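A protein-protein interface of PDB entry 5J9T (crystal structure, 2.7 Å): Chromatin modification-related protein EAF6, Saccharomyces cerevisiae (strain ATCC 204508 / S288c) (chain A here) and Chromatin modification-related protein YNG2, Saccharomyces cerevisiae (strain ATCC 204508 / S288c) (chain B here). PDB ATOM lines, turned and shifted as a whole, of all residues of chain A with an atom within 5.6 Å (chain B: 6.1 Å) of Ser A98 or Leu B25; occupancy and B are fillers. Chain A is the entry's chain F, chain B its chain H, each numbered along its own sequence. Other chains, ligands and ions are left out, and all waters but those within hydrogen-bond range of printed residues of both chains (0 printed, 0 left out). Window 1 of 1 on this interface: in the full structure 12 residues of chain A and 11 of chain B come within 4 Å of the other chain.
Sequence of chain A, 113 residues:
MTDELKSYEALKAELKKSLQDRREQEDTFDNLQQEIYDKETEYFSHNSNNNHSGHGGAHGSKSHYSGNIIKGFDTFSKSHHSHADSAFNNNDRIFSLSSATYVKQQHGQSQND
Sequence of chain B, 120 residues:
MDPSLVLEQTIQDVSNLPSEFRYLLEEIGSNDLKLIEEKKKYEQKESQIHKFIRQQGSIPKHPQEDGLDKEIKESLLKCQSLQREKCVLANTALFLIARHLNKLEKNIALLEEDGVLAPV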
ATOM      1  N   ARG A  93      -3.107   1.821  19.074  1.00  0.00           N
ATOM      2  CA  ARG A  93      -2.663   0.718  18.225  1.00  0.00           C
ATOM      3  C   ARG A  93      -3.855   0.097  17.494  1.00  0.00           C
ATOM      4  O   ARG A  93      -4.213  -1.059  17.698  1.00  0.00           O
ATOM      5  CB  ARG A  93      -1.944  -0.331  19.064  1.00  0.00           C
ATOM      6  CG  ARG A  93      -0.704   0.166  19.770  1.00  0.00           C
ATOM      7  CD  ARG A  93      -0.039  -0.960  20.536  1.00  0.00           C
ATOM      8  NE  ARG A  93       1.230  -0.542  21.117  1.00  0.00           N
ATOM      9  CZ  ARG A  93       2.395  -0.614  20.485  1.00  0.00           C
ATOM     10  NH1 ARG A  93       2.452  -1.090  19.247  1.00  0.00           N
ATOM     11  NH2 ARG A  93       3.503  -0.211  21.092  1.00  0.00           N
ATOM     12  N   ILE A  94      -4.447   0.886  16.596  1.00  0.00           N
ATOM     13  CA  ILE A  94      -5.666   0.458  15.927  1.00  0.00           C
ATOM     14  C   ILE A  94      -5.404  -0.731  15.019  1.00  0.00           C
ATOM     15  O   ILE A  94      -6.338  -1.469  14.687  1.00  0.00           O
ATOM     16  CB  ILE A  94      -6.281   1.625  15.135  1.00  0.00           C
ATOM     17  CG1 ILE A  94      -5.260   2.184  14.147  1.00  0.00           C
ATOM     18  CG2 ILE A  94      -6.803   2.697  16.077  1.00  0.00           C
ATOM     19  CD1 ILE A  94      -5.789   3.336  13.332  1.00  0.00           C
ATOM     20  N   PHE A  95      -4.150  -0.935  14.603  1.00  0.00           N
ATOM     21  CA  PHE A  95      -3.822  -2.047  13.717  1.00  0.00           C
ATOM     22  C   PHE A  95      -3.736  -3.363  14.482  1.00  0.00           C
ATOM     23  O   PHE A  95      -4.315  -4.373  14.062  1.00  0.00           O
ATOM     24  CB  PHE A  95      -2.511  -1.762  12.984  1.00  0.00           C
ATOM     25  CG  PHE A  95      -2.552  -0.524  12.143  1.00  0.00           C
ATOM     26  CD1 PHE A  95      -3.067  -0.560  10.858  1.00  0.00           C
ATOM     27  CD2 PHE A  95      -2.087   0.681  12.640  1.00  0.00           C
ATOM     28  CE1 PHE A  95      -3.112   0.584  10.086  1.00  0.00           C
ATOM     29  CE2 PHE A  95      -2.128   1.826  11.873  1.00  0.00           C
ATOM     30  CZ  PHE A  95      -2.640   1.777  10.593  1.00  0.00           C
ATOM     31  N   SER A  96      -3.014  -3.368  15.607  1.00  0.00           N
ATOM     32  CA  SER A  96      -2.958  -4.563  16.444  1.00  0.00           C
ATOM     33  C   SER A  96      -4.307  -4.848  17.083  1.00  0.00           C
ATOM     34  O   SER A  96      -4.688  -6.016  17.228  1.00  0.00           O
ATOM     35  CB  SER A  96      -1.877  -4.414  17.519  1.00  0.00           C
ATOM     36  OG  SER A  96      -0.578  -4.365  16.945  1.00  0.00           O
ATOM     37  N   LEU A  97      -5.038  -3.799  17.470  1.00  0.00           N
ATOM     38  CA  LEU A  97      -6.338  -3.954  18.103  1.00  0.00           C
ATOM     39  C   LEU A  97      -7.379  -4.532  17.156  1.00  0.00           C
ATOM     40  O   LEU A  97      -8.488  -4.833  17.602  1.00  0.00           O
ATOM     41  CB  LEU A  97      -6.811  -2.608  18.664  1.00  0.00           C
ATOM     42  CG  LEU A  97      -6.039  -2.134  19.907  1.00  0.00           C
ATOM     43  CD1 LEU A  97      -6.242  -0.646  20.155  1.00  0.00           C
ATOM     44  CD2 LEU A  97      -6.428  -2.931  21.139  1.00  0.00           C
ATOM     45  N   SER A  98      -7.063  -4.668  15.863  1.00  0.00           N
ATOM     46  CA  SER A  98      -7.978  -5.307  14.926  1.00  0.00           C
ATOM     47  C   SER A  98      -7.980  -6.812  15.081  1.00  0.00           C
ATOM     48  O   SER A  98      -8.904  -7.480  14.604  1.00  0.00           O
ATOM     49  CB  SER A  98      -7.595  -4.985  13.485  1.00  0.00           C
ATOM     50  OG  SER A  98      -7.384  -3.607  13.294  1.00  0.00           O
ATOM     51  N   SER A  99      -6.982  -7.350  15.760  1.00  0.00           N
ATOM     52  CA  SER A  99      -6.912  -8.772  16.044  1.00  0.00           C
ATOM     53  C   SER A  99      -7.431  -9.059  17.443  1.00  0.00           C
ATOM     54  O   SER A  99      -6.998  -8.430  18.412  1.00  0.00           O
ATOM     55  CB  SER A  99      -5.475  -9.278  15.919  1.00  0.00           C
ATOM     56  OG  SER A  99      -5.328 -10.629  16.346  1.00  0.00           O
ATOM     57  N   ALA A 100      -8.362  -9.998  17.547  1.00  0.00           N
ATOM     58  CA  ALA A 100      -8.870 -10.389  18.851  1.00  0.00           C
ATOM     59  C   ALA A 100      -7.856 -11.274  19.564  1.00  0.00           C
ATOM     60  O   ALA A 100      -7.996 -11.539  20.766  1.00  0.00           O
ATOM     61  CB  ALA A 100     -10.218 -11.101  18.688  1.00  0.00           C
ATOM     62  N   GLU B  20     -11.588   6.736   8.299  1.00  0.00           N
ATOM     63  CA  GLU B  20     -11.947   5.535   7.558  1.00  0.00           C
ATOM     64  C   GLU B  20     -11.092   4.348   7.980  1.00  0.00           C
ATOM     65  O   GLU B  20     -11.580   3.213   8.026  1.00  0.00           O
ATOM     66  CB  GLU B  20     -11.812   5.792   6.060  1.00  0.00           C
ATOM     67  CG  GLU B  20     -12.859   6.735   5.515  1.00  0.00           C
ATOM     68  CD  GLU B  20     -12.397   7.456   4.266  1.00  0.00           C
ATOM     69  OE1 GLU B  20     -11.272   7.184   3.793  1.00  0.00           O
ATOM     70  OE2 GLU B  20     -13.164   8.297   3.758  1.00  0.00           O
ATOM     71  N   PHE B  21      -9.813   4.587   8.273  1.00  0.00           N
ATOM     72  CA  PHE B  21      -8.962   3.516   8.778  1.00  0.00           C
ATOM     73  C   PHE B  21      -9.491   2.977  10.103  1.00  0.00           C
ATOM     74  O   PHE B  21      -9.627   1.761  10.281  1.00  0.00           O
ATOM     75  CB  PHE B  21      -7.527   4.014   8.923  1.00  0.00           C
ATOM     76  CG  PHE B  21      -6.627   3.599   7.795  1.00  0.00           C
ATOM     77  CD1 PHE B  21      -6.989   3.835   6.480  1.00  0.00           C
ATOM     78  CD2 PHE B  21      -5.415   2.981   8.050  1.00  0.00           C
ATOM     79  CE1 PHE B  21      -6.158   3.453   5.439  1.00  0.00           C
ATOM     80  CE2 PHE B  21      -4.581   2.601   7.016  1.00  0.00           C
ATOM     81  CZ  PHE B  21      -4.953   2.838   5.709  1.00  0.00           C
ATOM     82  N   ARG B  22      -9.815   3.872  11.038  1.00  0.00           N
ATOM     83  CA  ARG B  22     -10.390   3.439  12.310  1.00  0.00           C
ATOM     84  C   ARG B  22     -11.693   2.682  12.099  1.00  0.00           C
ATOM     85  O   ARG B  22     -11.916   1.627  12.705  1.00  0.00           O
ATOM     86  CB  ARG B  22     -10.624   4.651  13.215  1.00  0.00           C
ATOM     87  CG  ARG B  22      -9.393   5.106  13.966  1.00  0.00           C
ATOM     88  CD  ARG B  22      -9.729   6.240  14.907  1.00  0.00           C
ATOM     89  NE  ARG B  22      -8.574   6.633  15.705  1.00  0.00           N
ATOM     90  CZ  ARG B  22      -8.243   6.071  16.860  1.00  0.00           C
ATOM     91  NH1 ARG B  22      -8.987   5.094  17.360  1.00  0.00           N
ATOM     92  NH2 ARG B  22      -7.172   6.490  17.517  1.00  0.00           N
ATOM     93  N   TYR B  23     -12.559   3.200  11.227  1.00  0.00           N
ATOM     94  CA  TYR B  23     -13.859   2.579  10.991  1.00  0.00           C
ATOM     95  C   TYR B  23     -13.703   1.173  10.419  1.00  0.00           C
ATOM     96  O   TYR B  23     -14.373   0.231  10.858  1.00  0.00           O
ATOM     97  CB  TYR B  23     -14.679   3.473  10.063  1.00  0.00           C
ATOM     98  CG  TYR B  23     -16.067   2.975   9.746  1.00  0.00           C
ATOM     99  CD1 TYR B  23     -17.035   2.886  10.736  1.00  0.00           C
ATOM    100  CD2 TYR B  23     -16.422   2.634   8.448  1.00  0.00           C
ATOM    101  CE1 TYR B  23     -18.312   2.446  10.445  1.00  0.00           C
ATOM    102  CE2 TYR B  23     -17.694   2.195   8.148  1.00  0.00           C
ATOM    103  CZ  TYR B  23     -18.636   2.102   9.151  1.00  0.00           C
ATOM    104  OH  TYR B  23     -19.908   1.667   8.869  1.00  0.00           O
ATOM    105  N   LEU B  24     -12.817   1.014   9.434  1.00  0.00           N
ATOM    106  CA  LEU B  24     -12.588  -0.298   8.836  1.00  0.00           C
ATOM    107  C   LEU B  24     -11.912  -1.249   9.817  1.00  0.00           C
ATOM    108  O   LEU B  24     -12.320  -2.408   9.949  1.00  0.00           O
ATOM    109  CB  LEU B  24     -11.745  -0.145   7.569  1.00  0.00           C
ATOM    110  CG  LEU B  24     -12.420   0.569   6.394  1.00  0.00           C
ATOM    111  CD1 LEU B  24     -11.391   0.909   5.336  1.00  0.00           C
ATOM    112  CD2 LEU B  24     -13.518  -0.283   5.800  1.00  0.00           C
ATOM    113  N   LEU B  25     -10.888  -0.772  10.530  1.00  0.00           N
ATOM    114  CA  LEU B  25     -10.151  -1.642  11.442  1.00  0.00           C
ATOM    115  C   LEU B  25     -11.014  -2.130  12.604  1.00  0.00           C
ATOM    116  O   LEU B  25     -10.831  -3.261  13.066  1.00  0.00           O
ATOM    117  CB  LEU B  25      -8.906  -0.920  11.959  1.00  0.00           C
ATOM    118  CG  LEU B  25      -7.802  -0.767  10.905  1.00  0.00           C
ATOM    119  CD1 LEU B  25      -6.673   0.122  11.404  1.00  0.00           C
ATOM    120  CD2 LEU B  25      -7.272  -2.129  10.491  1.00  0.00           C
ATOM    121  N   GLU B  26     -11.957  -1.317  13.087  1.00  0.00           N
ATOM    122  CA  GLU B  26     -12.810  -1.792  14.172  1.00  0.00           C
ATOM    123  C   GLU B  26     -13.910  -2.715  13.672  1.00  0.00           C
ATOM    124  O   GLU B  26     -14.455  -3.494  14.462  1.00  0.00           O
ATOM    125  CB  GLU B  26     -13.428  -0.630  14.948  1.00  0.00           C
ATOM    126  CG  GLU B  26     -14.516   0.125  14.220  1.00  0.00           C
ATOM    127  CD  GLU B  26     -14.985   1.333  15.003  1.00  0.00           C
ATOM    128  OE1 GLU B  26     -14.494   1.533  16.134  1.00  0.00           O
ATOM    129  OE2 GLU B  26     -15.841   2.082  14.490  1.00  0.00           O
ATOM    130  N   GLU B  27     -14.245  -2.657  12.383  1.00  0.00           N
ATOM    131  CA  GLU B  27     -15.149  -3.655  11.836  1.00  0.00           C
ATOM    132  C   GLU B  27     -14.411  -4.971  11.639  1.00  0.00           C
ATOM    133  O   GLU B  27     -15.003  -6.045  11.800  1.00  0.00           O
ATOM    134  CB  GLU B  27     -15.748  -3.161  10.521  1.00  0.00           C
ATOM    135  CG  GLU B  27     -16.938  -2.230  10.704  1.00  0.00           C
ATOM    136  CD  GLU B  27     -18.036  -2.837  11.556  1.00  0.00           C
ATOM    137  OE1 GLU B  27     -18.459  -3.975  11.264  1.00  0.00           O
ATOM    138  OE2 GLU B  27     -18.473  -2.173  12.521  1.00  0.00           O
ATOM    139  N   ILE B  28     -13.117  -4.897  11.318  1.00  0.00           N
ATOM    140  CA  ILE B  28     -12.281  -6.089  11.300  1.00  0.00           C
ATOM    141  C   ILE B  28     -12.166  -6.661  12.705  1.00  0.00           C
ATOM    142  O   ILE B  28     -12.301  -7.873  12.914  1.00  0.00           O
ATOM    143  CB  ILE B  28     -10.895  -5.752  10.720  1.00  0.00           C
ATOM    144  CG1 ILE B  28     -10.989  -5.349   9.246  1.00  0.00           C
ATOM    145  CG2 ILE B  28      -9.955  -6.931  10.864  1.00  0.00           C
ATOM    146  CD1 ILE B  28      -9.647  -4.973   8.661  1.00  0.00           C
ATOM    147  N   GLY B  29     -11.950  -5.790  13.692  1.00  0.00           N
ATOM    148  CA  GLY B  29     -11.859  -6.243  15.070  1.00  0.00           C
ATOM    149  C   GLY B  29     -13.144  -6.879  15.559  1.00  0.00           C
ATOM    150  O   GLY B  29     -13.118  -7.899  16.251  1.00  0.00           O
ATOM    151  N   SER B  30     -14.286  -6.274  15.223  1.00  0.00           N
ATOM    152  CA  SER B  30     -15.565  -6.820  15.657  1.00  0.00           C
ATOM    153  C   SER B  30     -15.850  -8.159  14.991  1.00  0.00           C
ATOM    154  O   SER B  30     -16.487  -9.029  15.597  1.00  0.00           O
ATOM    155  CB  SER B  30     -16.688  -5.827  15.363  1.00  0.00           C
ATOM    156  OG  SER B  30     -17.940  -6.350  15.771  1.00  0.00           O
ATOM    157  N   ASP B  32     -13.386 -10.298  13.997  1.00  0.00           N
ATOM    158  CA  ASP B  32     -12.447 -11.268  14.549  1.00  0.00           C
ATOM    159  C   ASP B  32     -12.906 -11.779  15.907  1.00  0.00           C
ATOM    160  O   ASP B  32     -12.618 -12.927  16.262  1.00  0.00           O
ATOM    161  CB  ASP B  32     -11.051 -10.656  14.641  1.00  0.00           C
ATOM    162  CG  ASP B  32      -9.959 -11.706  14.709  1.00  0.00           C
ATOM    163  OD1 ASP B  32     -10.095 -12.753  14.039  1.00  0.00           O
ATOM    164  OD2 ASP B  32      -8.970 -11.491  15.441  1.00  0.00           O
ATOM    165  N   LYS B  86     -13.327  -9.886   6.593  1.00  0.00           N
ATOM    166  CA  LYS B  86     -12.168  -9.160   7.104  1.00  0.00           C
ATOM    167  C   LYS B  86     -11.157  -8.918   5.993  1.00  0.00           C
ATOM    168  O   LYS B  86     -10.518  -7.860   5.944  1.00  0.00           O
ATOM    169  CB  LYS B  86     -11.529  -9.929   8.263  1.00  0.00           C
ATOM    170  CG  LYS B  86     -12.529 -10.430   9.300  1.00  0.00           C
ATOM    171  CD  LYS B  86     -12.012 -10.277  10.719  1.00  0.00           C
ATOM    172  CE  LYS B  86     -10.679 -10.977  10.920  1.00  0.00           C
ATOM    173  NZ  LYS B  86     -10.757 -12.440  10.670  1.00  0.00           N
ATOM    174  N   ALA B  93      -9.029  -0.705   2.984  1.00  0.00           N
ATOM    175  CA  ALA B  93      -8.144   0.221   3.679  1.00  0.00           C
ATOM    176  C   ALA B  93      -6.822   0.348   2.938  1.00  0.00           C
ATOM    177  O   ALA B  93      -6.332   1.458   2.699  1.00  0.00           O
ATOM    178  CB  ALA B  93      -7.918  -0.236   5.121  1.00  0.00           C
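Printed residues of chain A that touch a printed residue of chain B: Ile A94, Phe A95, Ser A98, Ser A99 and Ala A100.
Hydrophobic or aromatic side chains of chain A that line the printed part of chain B: Ile A94, Phe A95 and Ala A100.
Among the printed residues, 10 pairs touch across the chains.
Among the printed residues, pairs that only touch across the chains: Ile A94 with Arg B22 (3.5 Å), Ile A94 with Leu B25 (3.7 Å), Phe A95 with Phe B21 (3.9 Å), Phe A95 with Leu B25 (3.7 Å), Ser A98 with Ile B28 (3.8 Å), Ser A98 with Gly B29 (3.2 Å), Ser A98 with Asp B32 (3.8 Å) and Ser A99 with Asp B32 (3.5 Å).
OG of Ser A98 lies within hydrogen-bond range of O of Ile A94 (2.8 Å).
O of Phe A95 sits at hydrogen-bond distance from OG of Ser A98 (3.3 Å).
The side-chain amino group of Lys B86 lies within salt-bridge range of the side-chain carboxylate of Asp B32, at 3.4 Å.
Ser A98 touches four residues of chain B.
Leu B25 touches just these residues of chain A: Ile A94 (3.7 Å), Phe A95 (3.7 Å) and Ser A98 (3.2 Å).
Of the printed residues of chain B, Ser A99 touches Asp B32.
Of the printed residues of chain B, Ile A94 touches Arg B22 and Leu B25.
Printed residues of chain B within 4 Å of Phe A95: Phe B21 and Leu B25.
Of the printed residues of chain A, Ile B28 touches Ser A98.
Tyr B23 touches none of the printed residues of chain A.
Leu B24 touches none of the printed residues of chain A.
The backbone carbonyl oxygen (O) of Leu B25 lies close to the side-chain hydroxyl (OG) of Ser A98, at 3.5 Å.
The side-chain carboxylate (OD2) of Asp B32 sits at hydrogen-bond distance from the backbone NH (N) of Ala A100 (2.7 Å).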
